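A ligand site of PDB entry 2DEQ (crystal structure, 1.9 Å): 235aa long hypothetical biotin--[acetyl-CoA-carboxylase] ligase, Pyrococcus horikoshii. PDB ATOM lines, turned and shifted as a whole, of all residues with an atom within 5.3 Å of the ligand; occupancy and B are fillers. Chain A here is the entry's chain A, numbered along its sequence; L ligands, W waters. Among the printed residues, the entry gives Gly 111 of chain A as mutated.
Water W4 bridges an oxygen (O8) of the ligand (2.9 Å) and the backbone NH (N) of Lys 52 (3.1 Å).
Water W1 lies within hydrogen-bond range of the side-chain amide oxygen of Asn 103 (2.8 Å), the guanidinium group of Arg 48 (2.9 Å), an oxygen (O4) of the ligand (3.2 Å) and the side-chain carboxylate of Asp 104 (3.4 Å).
The backbone carbonyl oxygen (O) of Ile 128 lies close to a sulfur (S1) of the ligand (3.7 Å).
OD1 of Asn 23 touches C8 of the ligand (3.5 Å).
CA of Gly 45 touches O3 of the ligand, at 3.5 Å.
CA of Gly 47 touches O1 of the ligand, 3.2 Å away.
Lys 52 touches the ligand.
CZ3 of Trp 53 touches C20 of the ligand (3.3 Å).
O of Leu 62 touches C7 of the ligand (3.3 Å).
Ser 63 touches the ligand (OG to C8, 3.8 Å).
Gly 111 touches the ligand.
CA of Gly 114 touches O2 of the ligand, 3.3 Å away.
Val 115 touches the ligand (N to C2, 3.8 Å).
Leu 116 touches the ligand.
Gly 129 touches the ligand.
Pro 137 touches the ligand.
CB of Ala 140 touches C19 of the ligand, 3.3 Å away.
Hydrophobic or aromatic side chains within 4 Å of the ligand: His 46, Trp 53, Leu 116, Pro 137 and Ala 140.
Along chain A the residues within 4 Å of the ligand span positions 21 to 140.
The nearest printed residue that does not touch the ligand is Trp 61 (4.03 Å).
N of Glu 54 sits at hydrogen-bond distance from N4 of the ligand.
An oxygen (O4) of the ligand sits at hydrogen-bond distance from the side-chain amide nitrogen (ND2) of Asn 103 (2.9 Å).
The side-chain carboxylate (OD1) of Asp 104 sits close to an oxygen (O4) of the ligand.
The guanidinium group (NH1) of Arg 51 lies within salt-bridge range of an oxygen (O5) of the ligand (2.8 Å).
The backbone NH (N) of His 46 is in hydrogen-bond range of an oxygen (O3) of the ligand, at 3.0 Å.
The side-chain amide nitrogen of Asn 131 sits at hydrogen-bond distance from a nitrogen (N6) of the ligand (2.7 Å).
The backbone carbonyl oxygen (O) of Glu 54 sits at hydrogen-bond distance from a nitrogen (N5) of the ligand (2.9 Å).
The side-chain amide oxygen (OE1) of Gln 42 is in hydrogen-bond range of a nitrogen (N1) of the ligand, at 3.0 Å.
O1 of the ligand sits at hydrogen-bond distance from N of Arg 48.
The side-chain hydroxyl (OG) of Ser 21 is in hydrogen-bond range of an oxygen (O3) of the ligand (2.7 Å).
N2 of the ligand is in hydrogen-bond range of O of His 46 (2.9 Å).
The side-chain hydroxyl (OG1) of Thr 22 lies within hydrogen-bond range of a nitrogen (N1) of the ligand (3.1 Å).
OE1 of Gln 42 sits at hydrogen-bond distance from N of Thr 22 (2.9 Å).
The backbone carbonyl oxygen (O) of Leu 116 is in hydrogen-bond range of the side-chain amide nitrogen (ND2) of Asn 23 (3.3 Å).
The side-chain amide nitrogen (ND2) of Asn 134 sits at hydrogen-bond distance from the side-chain amide oxygen (OD1) of Asn 131.
The side-chain hydroxyl of Ser 21 lies close to the backbone NH of Asn 23 (3.3 Å).
The backbone NH (N) of Trp 53 sits at hydrogen-bond distance from the backbone carbonyl oxygen (O) of Gly 45 (3.0 Å).
O of Asn 103 sits at hydrogen-bond distance from N of Val 115 (2.9 Å).
The backbone carbonyl oxygen (O) of Leu 62 sits at hydrogen-bond distance from the backbone NH (N) of Ile 128, 2.8 Å away.
N of Leu 116 lies within hydrogen-bond range of O of Gly 127 (2.8 Å).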
ATOM      1  N   SER A  21       7.356 -16.593   7.837  1.00  0.00           N
ATOM      2  CA  SER A  21       8.369 -16.658   8.892  1.00  0.00           C
ATOM      3  C   SER A  21       7.783 -16.131  10.201  1.00  0.00           C
ATOM      4  O   SER A  21       7.232 -15.029  10.234  1.00  0.00           O
ATOM      5  CB  SER A  21       9.584 -15.828   8.511  1.00  0.00           C
ATOM      6  OG  SER A  21      10.475 -15.708   9.595  1.00  0.00           O
ATOM      7  N   THR A  22       7.902 -16.898  11.277  1.00  0.00           N
ATOM      8  CA  THR A  22       7.386 -16.461  12.567  1.00  0.00           C
ATOM      9  C   THR A  22       8.157 -15.219  13.051  1.00  0.00           C
ATOM     10  O   THR A  22       7.593 -14.339  13.709  1.00  0.00           O
ATOM     11  CB  THR A  22       7.491 -17.577  13.637  1.00  0.00           C
ATOM     12  OG1 THR A  22       8.857 -17.971  13.811  1.00  0.00           O
ATOM     13  CG2 THR A  22       6.653 -18.777  13.219  1.00  0.00           C
ATOM     14  N   ASN A  23       9.449 -15.139  12.730  1.00  0.00           N
ATOM     15  CA  ASN A  23      10.228 -13.976  13.164  1.00  0.00           C
ATOM     16  C   ASN A  23       9.767 -12.711  12.448  1.00  0.00           C
ATOM     17  O   ASN A  23       9.652 -11.655  13.071  1.00  0.00           O
ATOM     18  CB  ASN A  23      11.721 -14.202  12.902  1.00  0.00           C
ATOM     19  CG  ASN A  23      12.503 -14.441  14.177  1.00  0.00           C
ATOM     20  OD1 ASN A  23      12.054 -15.171  15.067  1.00  0.00           O
ATOM     21  ND2 ASN A  23      13.682 -13.840  14.283  1.00  0.00           N
ATOM     22  N   GLN A  42       7.227 -23.205   7.765  1.00  0.00           N
ATOM     23  CA  GLN A  42       7.549 -21.865   7.290  1.00  0.00           C
ATOM     24  C   GLN A  42       7.994 -22.009   5.843  1.00  0.00           C
ATOM     25  O   GLN A  42       8.731 -22.943   5.514  1.00  0.00           O
ATOM     26  CB  GLN A  42       8.686 -21.244   8.102  1.00  0.00           C
ATOM     27  CG  GLN A  42       8.428 -21.088   9.588  1.00  0.00           C
ATOM     28  CD  GLN A  42       9.571 -20.375  10.312  1.00  0.00           C
ATOM     29  OE1 GLN A  42       9.384 -19.313  10.904  1.00  0.00           O
ATOM     30  NE2 GLN A  42      10.754 -20.966  10.265  1.00  0.00           N
ATOM     31  N   MET A  44       9.450 -19.320   4.255  1.00  0.00           N
ATOM     32  CA  MET A  44      10.618 -18.437   4.132  1.00  0.00           C
ATOM     33  C   MET A  44      11.372 -18.328   5.450  1.00  0.00           C
ATOM     34  O   MET A  44      11.685 -17.228   5.905  1.00  0.00           O
ATOM     35  CB  MET A  44      10.170 -17.039   3.685  1.00  0.00           C
ATOM     36  CG  MET A  44       9.365 -17.012   2.403  1.00  0.00           C
ATOM     37  SD  MET A  44       8.932 -15.328   1.901  1.00  0.00           S
ATOM     38  CE  MET A  44      10.504 -14.772   1.215  1.00  0.00           C
ATOM     39  N   GLY A  45      11.649 -19.466   6.073  1.00  0.00           N
ATOM     40  CA  GLY A  45      12.365 -19.436   7.340  1.00  0.00           C
ATOM     41  C   GLY A  45      13.789 -18.965   7.136  1.00  0.00           C
ATOM     42  O   GLY A  45      14.406 -19.283   6.119  1.00  0.00           O
ATOM     43  N   HIS A  46      14.317 -18.182   8.066  1.00  0.00           N
ATOM     44  CA  HIS A  46      15.704 -17.765   7.912  1.00  0.00           C
ATOM     45  C   HIS A  46      16.563 -17.790   9.172  1.00  0.00           C
ATOM     46  O   HIS A  46      16.063 -17.766  10.301  1.00  0.00           O
ATOM     47  CB  HIS A  46      15.801 -16.374   7.258  1.00  0.00           C
ATOM     48  CG  HIS A  46      15.047 -15.290   7.976  1.00  0.00           C
ATOM     49  ND1 HIS A  46      13.710 -15.055   7.750  1.00  0.00           N
ATOM     50  CD2 HIS A  46      15.451 -14.361   8.875  1.00  0.00           C
ATOM     51  CE1 HIS A  46      13.318 -14.029   8.491  1.00  0.00           C
ATOM     52  NE2 HIS A  46      14.356 -13.587   9.185  1.00  0.00           N
ATOM     53  N   GLY A  47      17.869 -17.858   8.937  1.00  0.00           N
ATOM     54  CA  GLY A  47      18.826 -17.860  10.016  1.00  0.00           C
ATOM     55  C   GLY A  47      19.501 -16.503   9.991  1.00  0.00           C
ATOM     56  O   GLY A  47      18.873 -15.506   9.625  1.00  0.00           O
ATOM     57  N   ARG A  48      20.768 -16.456  10.361  1.00  0.00           N
ATOM     58  CA  ARG A  48      21.499 -15.200  10.353  1.00  0.00           C
ATOM     59  C   ARG A  48      21.892 -14.827   8.929  1.00  0.00           C
ATOM     60  O   ARG A  48      22.242 -15.695   8.125  1.00  0.00           O
ATOM     61  CB  ARG A  48      22.754 -15.342  11.230  1.00  0.00           C
ATOM     62  CG  ARG A  48      22.459 -15.876  12.618  1.00  0.00           C
ATOM     63  CD  ARG A  48      23.745 -16.184  13.366  1.00  0.00           C
ATOM     64  NE  ARG A  48      24.569 -14.989  13.534  1.00  0.00           N
ATOM     65  CZ  ARG A  48      25.858 -15.002  13.870  1.00  0.00           C
ATOM     66  NH1 ARG A  48      26.478 -16.161  14.062  1.00  0.00           N
ATOM     67  NH2 ARG A  48      26.517 -13.863  13.991  1.00  0.00           N
ATOM     68  N   ARG A  51      20.205 -16.354   5.755  1.00  0.00           N
ATOM     69  CA  ARG A  51      20.598 -17.686   5.319  1.00  0.00           C
ATOM     70  C   ARG A  51      19.258 -18.399   5.433  1.00  0.00           C
ATOM     71  O   ARG A  51      18.402 -17.984   6.210  1.00  0.00           O
ATOM     72  CB  ARG A  51      21.575 -18.317   6.307  1.00  0.00           C
ATOM     73  CG  ARG A  51      23.007 -17.792   6.249  1.00  0.00           C
ATOM     74  CD  ARG A  51      23.750 -18.190   7.512  1.00  0.00           C
ATOM     75  NE  ARG A  51      25.169 -17.829   7.450  1.00  0.00           N
ATOM     76  CZ  ARG A  51      25.975 -17.828   8.503  1.00  0.00           C
ATOM     77  NH1 ARG A  51      25.510 -18.139   9.710  1.00  0.00           N
ATOM     78  NH2 ARG A  51      27.254 -17.506   8.358  1.00  0.00           N
ATOM     79  N   LYS A  52      19.032 -19.462   4.663  1.00  0.00           N
ATOM     80  CA  LYS A  52      17.755 -20.145   4.766  1.00  0.00           C
ATOM     81  C   LYS A  52      17.736 -21.180   5.870  1.00  0.00           C
ATOM     82  O   LYS A  52      18.730 -21.850   6.121  1.00  0.00           O
ATOM     83  CB  LYS A  52      17.373 -20.836   3.453  1.00  0.00           C
ATOM     84  CG  LYS A  52      16.047 -21.597   3.581  1.00  0.00           C
ATOM     85  CD  LYS A  52      15.593 -22.154   2.254  1.00  0.00           C
ATOM     86  CE  LYS A  52      14.109 -21.879   2.098  1.00  0.00           C
ATOM     87  NZ  LYS A  52      13.417 -22.400   3.317  1.00  0.00           N
ATOM     88  N   TRP A  53      16.587 -21.278   6.540  1.00  0.00           N
ATOM     89  CA  TRP A  53      16.392 -22.263   7.589  1.00  0.00           C
ATOM     90  C   TRP A  53      15.241 -23.161   7.099  1.00  0.00           C
ATOM     91  O   TRP A  53      14.121 -22.695   6.927  1.00  0.00           O
ATOM     92  CB  TRP A  53      16.005 -21.601   8.915  1.00  0.00           C
ATOM     93  CG  TRP A  53      15.819 -22.579  10.031  1.00  0.00           C
ATOM     94  CD1 TRP A  53      14.639 -23.113  10.460  1.00  0.00           C
ATOM     95  CD2 TRP A  53      16.850 -23.191  10.808  1.00  0.00           C
ATOM     96  NE1 TRP A  53      14.877 -24.037  11.470  1.00  0.00           N
ATOM     97  CE2 TRP A  53      16.232 -24.094  11.695  1.00  0.00           C
ATOM     98  CE3 TRP A  53      18.251 -23.067  10.843  1.00  0.00           C
ATOM     99  CZ2 TRP A  53      16.958 -24.874  12.604  1.00  0.00           C
ATOM    100  CZ3 TRP A  53      18.972 -23.839  11.748  1.00  0.00           C
ATOM    101  CH2 TRP A  53      18.324 -24.728  12.621  1.00  0.00           C
ATOM    102  N   GLU A  54      15.540 -24.436   6.862  1.00  0.00           N
ATOM    103  CA  GLU A  54      14.515 -25.378   6.378  1.00  0.00           C
ATOM    104  C   GLU A  54      13.504 -25.586   7.507  1.00  0.00           C
ATOM    105  O   GLU A  54      13.877 -26.001   8.612  1.00  0.00           O
ATOM    106  CB  GLU A  54      15.155 -26.722   6.018  1.00  0.00           C
ATOM    107  CG  GLU A  54      16.261 -26.664   4.960  1.00  0.00           C
ATOM    108  CD  GLU A  54      15.729 -26.303   3.572  1.00  0.00           C
ATOM    109  OE1 GLU A  54      14.622 -26.752   3.206  1.00  0.00           O
ATOM    110  OE2 GLU A  54      16.431 -25.569   2.843  1.00  0.00           O
ATOM    111  N   SER A  55      12.227 -25.321   7.213  1.00  0.00           N
ATOM    112  CA  SER A  55      11.177 -25.441   8.223  1.00  0.00           C
ATOM    113  C   SER A  55      10.001 -26.311   7.804  1.00  0.00           C
ATOM    114  O   SER A  55       8.874 -25.830   7.702  1.00  0.00           O
ATOM    115  CB  SER A  55      10.666 -24.043   8.577  1.00  0.00           C
ATOM    116  OG  SER A  55      11.746 -23.150   8.803  1.00  0.00           O
ATOM    117  N   TRP A  61       8.851 -24.464  15.072  1.00  0.00           N
ATOM    118  CA  TRP A  61       9.300 -23.173  14.549  1.00  0.00           C
ATOM    119  C   TRP A  61       8.503 -22.092  15.281  1.00  0.00           C
ATOM    120  O   TRP A  61       7.286 -21.974  15.094  1.00  0.00           O
ATOM    121  CB  TRP A  61       9.013 -23.101  13.040  1.00  0.00           C
ATOM    122  CG  TRP A  61       9.172 -24.431  12.331  1.00  0.00           C
ATOM    123  CD1 TRP A  61       8.225 -25.085  11.591  1.00  0.00           C
ATOM    124  CD2 TRP A  61      10.352 -25.249  12.278  1.00  0.00           C
ATOM    125  NE1 TRP A  61       8.746 -26.258  11.086  1.00  0.00           N
ATOM    126  CE2 TRP A  61      10.049 -26.379  11.488  1.00  0.00           C
ATOM    127  CE3 TRP A  61      11.643 -25.132  12.824  1.00  0.00           C
ATOM    128  CZ2 TRP A  61      10.982 -27.398  11.223  1.00  0.00           C
ATOM    129  CZ3 TRP A  61      12.574 -26.147  12.568  1.00  0.00           C
ATOM    130  CH2 TRP A  61      12.238 -27.260  11.773  1.00  0.00           C
ATOM    131  N   LEU A  62       9.166 -21.329  16.140  1.00  0.00           N
ATOM    132  CA  LEU A  62       8.456 -20.302  16.896  1.00  0.00           C
ATOM    133  C   LEU A  62       9.270 -19.042  17.178  1.00  0.00           C
ATOM    134  O   LEU A  62      10.496 -19.042  17.084  1.00  0.00           O
ATOM    135  CB  LEU A  62       7.937 -20.908  18.220  1.00  0.00           C
ATOM    136  CG  LEU A  62       8.965 -21.486  19.206  1.00  0.00           C
ATOM    137  CD1 LEU A  62       9.595 -20.370  20.035  1.00  0.00           C
ATOM    138  CD2 LEU A  62       8.254 -22.468  20.132  1.00  0.00           C
ATOM    139  N   SER A  63       8.554 -17.979  17.530  1.00  0.00           N
ATOM    140  CA  SER A  63       9.166 -16.701  17.857  1.00  0.00           C
ATOM    141  C   SER A  63       8.463 -16.153  19.095  1.00  0.00           C
ATOM    142  O   SER A  63       7.252 -16.346  19.262  1.00  0.00           O
ATOM    143  CB  SER A  63       9.025 -15.709  16.702  1.00  0.00           C
ATOM    144  OG  SER A  63       9.705 -16.171  15.542  1.00  0.00           O
ATOM    145  N   ASN A 103      24.606 -19.127  18.928  1.00  0.00           N
ATOM    146  CA  ASN A 103      23.155 -19.335  18.716  1.00  0.00           C
ATOM    147  C   ASN A 103      22.751 -20.788  18.318  1.00  0.00           C
ATOM    148  O   ASN A 103      21.587 -21.085  18.082  1.00  0.00           O
ATOM    149  CB  ASN A 103      22.676 -18.345  17.652  1.00  0.00           C
ATOM    150  CG  ASN A 103      23.274 -18.724  16.320  1.00  0.00           C
ATOM    151  OD1 ASN A 103      24.452 -19.035  16.205  1.00  0.00           O
ATOM    152  ND2 ASN A 103      22.411 -18.705  15.289  1.00  0.00           N
ATOM    153  N   ASP A 104      23.692 -21.712  18.180  1.00  0.00           N
ATOM    154  CA  ASP A 104      23.330 -23.037  17.719  1.00  0.00           C
ATOM    155  C   ASP A 104      23.404 -24.119  18.788  1.00  0.00           C
ATOM    156  O   ASP A 104      24.196 -24.031  19.740  1.00  0.00           O
ATOM    157  CB  ASP A 104      24.224 -23.454  16.544  1.00  0.00           C
ATOM    158  CG  ASP A 104      24.144 -22.490  15.371  1.00  0.00           C
ATOM    159  OD1 ASP A 104      23.026 -22.101  14.987  1.00  0.00           O
ATOM    160  OD2 ASP A 104      25.207 -22.124  14.836  1.00  0.00           O
ATOM    161  N   GLY A 111      23.713 -30.220  13.870  1.00  0.00           N
ATOM    162  CA  GLY A 111      22.744 -29.193  14.224  1.00  0.00           C
ATOM    163  C   GLY A 111      21.330 -29.683  14.451  1.00  0.00           C
ATOM    164  O   GLY A 111      20.728 -30.306  13.575  1.00  0.00           O
ATOM    165  N   ILE A 112      20.794 -29.402  15.630  1.00  0.00           N
ATOM    166  CA  ILE A 112      19.435 -29.819  15.948  1.00  0.00           C
ATOM    167  C   ILE A 112      18.524 -28.611  16.162  1.00  0.00           C
ATOM    168  O   ILE A 112      17.300 -28.728  16.086  1.00  0.00           O
ATOM    169  CB  ILE A 112      19.400 -30.735  17.196  1.00  0.00           C
ATOM    170  CG1 ILE A 112      18.047 -31.447  17.260  1.00  0.00           C
ATOM    171  CG2 ILE A 112      19.629 -29.910  18.465  1.00  0.00           C
ATOM    172  CD1 ILE A 112      17.977 -32.536  18.321  1.00  0.00           C
ATOM    173  N   ALA A 113      19.125 -27.444  16.403  1.00  0.00           N
ATOM    174  CA  ALA A 113      18.356 -26.225  16.635  1.00  0.00           C
ATOM    175  C   ALA A 113      19.167 -24.958  16.402  1.00  0.00           C
ATOM    176  O   ALA A 113      20.398 -24.960  16.469  1.00  0.00           O
ATOM    177  CB  ALA A 113      17.787 -26.230  18.055  1.00  0.00           C
ATOM    178  N   GLY A 114      18.467 -23.865  16.131  1.00  0.00           N
ATOM    179  CA  GLY A 114      19.127 -22.593  15.917  1.00  0.00           C
ATOM    180  C   GLY A 114      18.301 -21.464  16.518  1.00  0.00           C
ATOM    181  O   GLY A 114      17.067 -21.557  16.552  1.00  0.00           O
ATOM    182  N   VAL A 115      18.971 -20.415  16.969  1.00  0.00           N
ATOM    183  CA  VAL A 115      18.319 -19.269  17.591  1.00  0.00           C
ATOM    184  C   VAL A 115      18.632 -17.988  16.836  1.00  0.00           C
ATOM    185  O   VAL A 115      19.785 -17.714  16.492  1.00  0.00           O
ATOM    186  CB  VAL A 115      18.762 -19.105  19.069  1.00  0.00           C
ATOM    187  CG1 VAL A 115      18.009 -17.961  19.737  1.00  0.00           C
ATOM    188  CG2 VAL A 115      18.514 -20.422  19.834  1.00  0.00           C
ATOM    189  N   LEU A 116      17.603 -17.190  16.572  1.00  0.00           N
ATOM    190  CA  LEU A 116      17.783 -15.934  15.854  1.00  0.00           C
ATOM    191  C   LEU A 116      17.048 -14.820  16.563  1.00  0.00           C
ATOM    192  O   LEU A 116      15.824 -14.824  16.648  1.00  0.00           O
ATOM    193  CB  LEU A 116      17.247 -16.050  14.432  1.00  0.00           C
ATOM    194  CG  LEU A 116      17.275 -14.747  13.633  1.00  0.00           C
ATOM    195  CD1 LEU A 116      18.717 -14.356  13.324  1.00  0.00           C
ATOM    196  CD2 LEU A 116      16.480 -14.927  12.340  1.00  0.00           C
ATOM    197  N   GLY A 127      13.661 -15.854  18.135  1.00  0.00           N
ATOM    198  CA  GLY A 127      13.220 -16.924  17.250  1.00  0.00           C
ATOM    199  C   GLY A 127      13.990 -18.209  17.505  1.00  0.00           C
ATOM    200  O   GLY A 127      15.210 -18.189  17.661  1.00  0.00           O
ATOM    201  N   ILE A 128      13.263 -19.325  17.526  1.00  0.00           N
ATOM    202  CA  ILE A 128      13.860 -20.627  17.782  1.00  0.00           C
ATOM    203  C   ILE A 128      13.343 -21.685  16.816  1.00  0.00           C
ATOM    204  O   ILE A 128      12.138 -21.840  16.638  1.00  0.00           O
ATOM    205  CB  ILE A 128      13.553 -21.094  19.226  1.00  0.00           C
ATOM    206  CG1 ILE A 128      14.007 -20.023  20.227  1.00  0.00           C
ATOM    207  CG2 ILE A 128      14.250 -22.433  19.500  1.00  0.00           C
ATOM    208  CD1 ILE A 128      13.693 -20.373  21.680  1.00  0.00           C
ATOM    209  N   GLY A 129      14.272 -22.397  16.188  1.00  0.00           N
ATOM    210  CA  GLY A 129      13.921 -23.465  15.267  1.00  0.00           C
ATOM    211  C   GLY A 129      14.515 -24.749  15.830  1.00  0.00           C
ATOM    212  O   GLY A 129      15.724 -24.810  16.056  1.00  0.00           O
ATOM    213  N   ASN A 131      14.504 -29.074  15.382  1.00  0.00           N
ATOM    214  CA  ASN A 131      14.100 -30.249  14.613  1.00  0.00           C
ATOM    215  C   ASN A 131      13.578 -31.327  15.550  1.00  0.00           C
ATOM    216  O   ASN A 131      14.301 -31.809  16.418  1.00  0.00           O
ATOM    217  CB  ASN A 131      15.281 -30.804  13.799  1.00  0.00           C
ATOM    218  CG  ASN A 131      15.817 -29.817  12.784  1.00  0.00           C
ATOM    219  OD1 ASN A 131      15.044 -29.196  12.042  1.00  0.00           O
ATOM    220  ND2 ASN A 131      17.137 -29.673  12.735  1.00  0.00           N
ATOM    221  N   ASN A 134      10.581 -33.710  11.930  1.00  0.00           N
ATOM    222  CA  ASN A 134      10.750 -33.362  10.522  1.00  0.00           C
ATOM    223  C   ASN A 134      12.002 -33.915   9.860  1.00  0.00           C
ATOM    224  O   ASN A 134      12.959 -34.291  10.540  1.00  0.00           O
ATOM    225  CB  ASN A 134      10.791 -31.848  10.373  1.00  0.00           C
ATOM    226  CG  ASN A 134      11.828 -31.207  11.288  1.00  0.00           C
ATOM    227  OD1 ASN A 134      11.653 -31.192  12.509  1.00  0.00           O
ATOM    228  ND2 ASN A 134      12.900 -30.689  10.716  1.00  0.00           N
ATOM    229  N   VAL A 136      15.415 -33.448   7.930  1.00  0.00           N
ATOM    230  CA  VAL A 136      16.381 -32.370   8.074  1.00  0.00           C
ATOM    231  C   VAL A 136      17.460 -32.368   6.992  1.00  0.00           C
ATOM    232  O   VAL A 136      17.637 -33.353   6.281  1.00  0.00           O
ATOM    233  CB  VAL A 136      17.096 -32.459   9.444  1.00  0.00           C
ATOM    234  CG1 VAL A 136      16.052 -32.481  10.567  1.00  0.00           C
ATOM    235  CG2 VAL A 136      17.961 -33.718   9.505  1.00  0.00           C
ATOM    236  N   PRO A 137      18.162 -31.234   6.831  1.00  0.00           N
ATOM    237  CA  PRO A 137      19.227 -31.141   5.826  1.00  0.00           C
ATOM    238  C   PRO A 137      20.326 -32.148   6.173  1.00  0.00           C
ATOM    239  O   PRO A 137      20.446 -32.556   7.327  1.00  0.00           O
ATOM    240  CB  PRO A 137      19.712 -29.699   5.965  1.00  0.00           C
ATOM    241  CG  PRO A 137      18.510 -28.970   6.487  1.00  0.00           C
ATOM    242  CD  PRO A 137      17.941 -29.939   7.496  1.00  0.00           C
ATOM    243  N   ALA A 140      22.488 -32.243   9.614  1.00  0.00           N
ATOM    244  CA  ALA A 140      21.691 -31.861  10.772  1.00  0.00           C
ATOM    245  C   ALA A 140      21.087 -33.115  11.389  1.00  0.00           C
ATOM    246  O   ALA A 140      21.289 -34.223  10.878  1.00  0.00           O
ATOM    247  CB  ALA A 140      20.574 -30.907  10.355  1.00  0.00           C
ATOM    248  N   THR A 141      20.366 -32.958  12.491  1.00  0.00           N
ATOM    249  CA  THR A 141      19.731 -34.091  13.144  1.00  0.00           C
ATOM    250  C   THR A 141      18.426 -33.628  13.814  1.00  0.00           C
ATOM    251  O   THR A 141      18.081 -32.447  13.767  1.00  0.00           O
ATOM    252  CB  THR A 141      20.668 -34.752  14.183  1.00  0.00           C
ATOM    253  OG1 THR A 141      20.073 -35.966  14.645  1.00  0.00           O
ATOM    254  CG2 THR A 141      20.924 -33.833  15.368  1.00  0.00           C
HETATM  255  C1  LIG L   1      20.232 -20.114  12.837  1.00  0.00           C
HETATM  256  O1  LIG L   1      20.931 -19.361  11.951  1.00  0.00           O
HETATM  257  O2  LIG L   1      20.650 -21.182  13.301  1.00  0.00           O
HETATM  258  C2  LIG L   1      18.980 -19.656  13.238  1.00  0.00           C
HETATM  259  C3  LIG L   1      17.823 -20.248  12.748  1.00  0.00           C
HETATM  260  C4  LIG L   1      16.567 -19.667  13.395  1.00  0.00           C
HETATM  261  C5  LIG L   1      15.312 -20.334  12.827  1.00  0.00           C
HETATM  262  C6  LIG L   1      14.041 -19.931  13.579  1.00  0.00           C
HETATM  263  S1  LIG L   1      12.559 -20.868  13.074  1.00  0.00           S
HETATM  264  C7  LIG L   1      11.470 -19.705  13.970  1.00  0.00           C
HETATM  265  C8  LIG L   1      12.090 -18.342  13.623  1.00  0.00           C
HETATM  266  N1  LIG L   1      11.567 -17.912  12.318  1.00  0.00           N
HETATM  267  C9  LIG L   1      12.565 -17.815  11.443  1.00  0.00           C
HETATM  268  O3  LIG L   1      12.411 -17.493  10.265  1.00  0.00           O
HETATM  269  N2  LIG L   1      13.763 -18.117  11.963  1.00  0.00           N
HETATM  270  C10 LIG L   1      13.604 -18.480  13.380  1.00  0.00           C
HETATM  271  P1  LIG L   1      22.414 -19.905  11.646  1.00  0.00           P
HETATM  272  O4  LIG L   1      23.115 -20.183  12.910  1.00  0.00           O
HETATM  273  O5  LIG L   1      23.020 -18.919  10.716  1.00  0.00           O
HETATM  274  O6  LIG L   1      22.209 -21.282  10.851  1.00  0.00           O
HETATM  275  C11 LIG L   1      21.950 -21.279   9.438  1.00  0.00           C
HETATM  276  C12 LIG L   1      22.312 -22.623   8.818  1.00  0.00           C
HETATM  277  O7  LIG L   1      21.690 -23.717   9.501  1.00  0.00           O
HETATM  278  C13 LIG L   1      21.801 -22.746   7.383  1.00  0.00           C
HETATM  279  O8  LIG L   1      22.690 -22.026   6.524  1.00  0.00           O
HETATM  280  C14 LIG L   1      22.016 -24.243   7.199  1.00  0.00           C
HETATM  281  O9  LIG L   1      23.407 -24.509   6.988  1.00  0.00           O
HETATM  282  C15 LIG L   1      21.588 -24.805   8.557  1.00  0.00           C
HETATM  283  N3  LIG L   1      20.177 -25.243   8.590  1.00  0.00           N
HETATM  284  C16 LIG L   1      19.174 -24.787   7.850  1.00  0.00           C
HETATM  285  N4  LIG L   1      18.043 -25.393   8.223  1.00  0.00           N
HETATM  286  C17 LIG L   1      18.334 -26.248   9.212  1.00  0.00           C
HETATM  287  C18 LIG L   1      17.564 -27.105   9.972  1.00  0.00           C
HETATM  288  N5  LIG L   1      16.248 -27.184   9.765  1.00  0.00           N
HETATM  289  N6  LIG L   1      18.143 -27.905  10.959  1.00  0.00           N
HETATM  290  C19 LIG L   1      19.594 -27.883  11.270  1.00  0.00           C
HETATM  291  N7  LIG L   1      20.333 -26.908  10.435  1.00  0.00           N
HETATM  292  C20 LIG L   1      19.707 -26.148   9.445  1.00  0.00           C
HETATM  293  O   HOH W   1      25.973 -18.995  13.894  1.00  0.00           O
HETATM  294  O   HOH W   2      25.349 -25.270   8.881  1.00  0.00           O
HETATM  295  O   HOH W   3      22.873 -26.292  11.810  1.00  0.00           O
HETATM  296  O   HOH W   4      21.549 -21.237   4.014  1.00  0.00           O
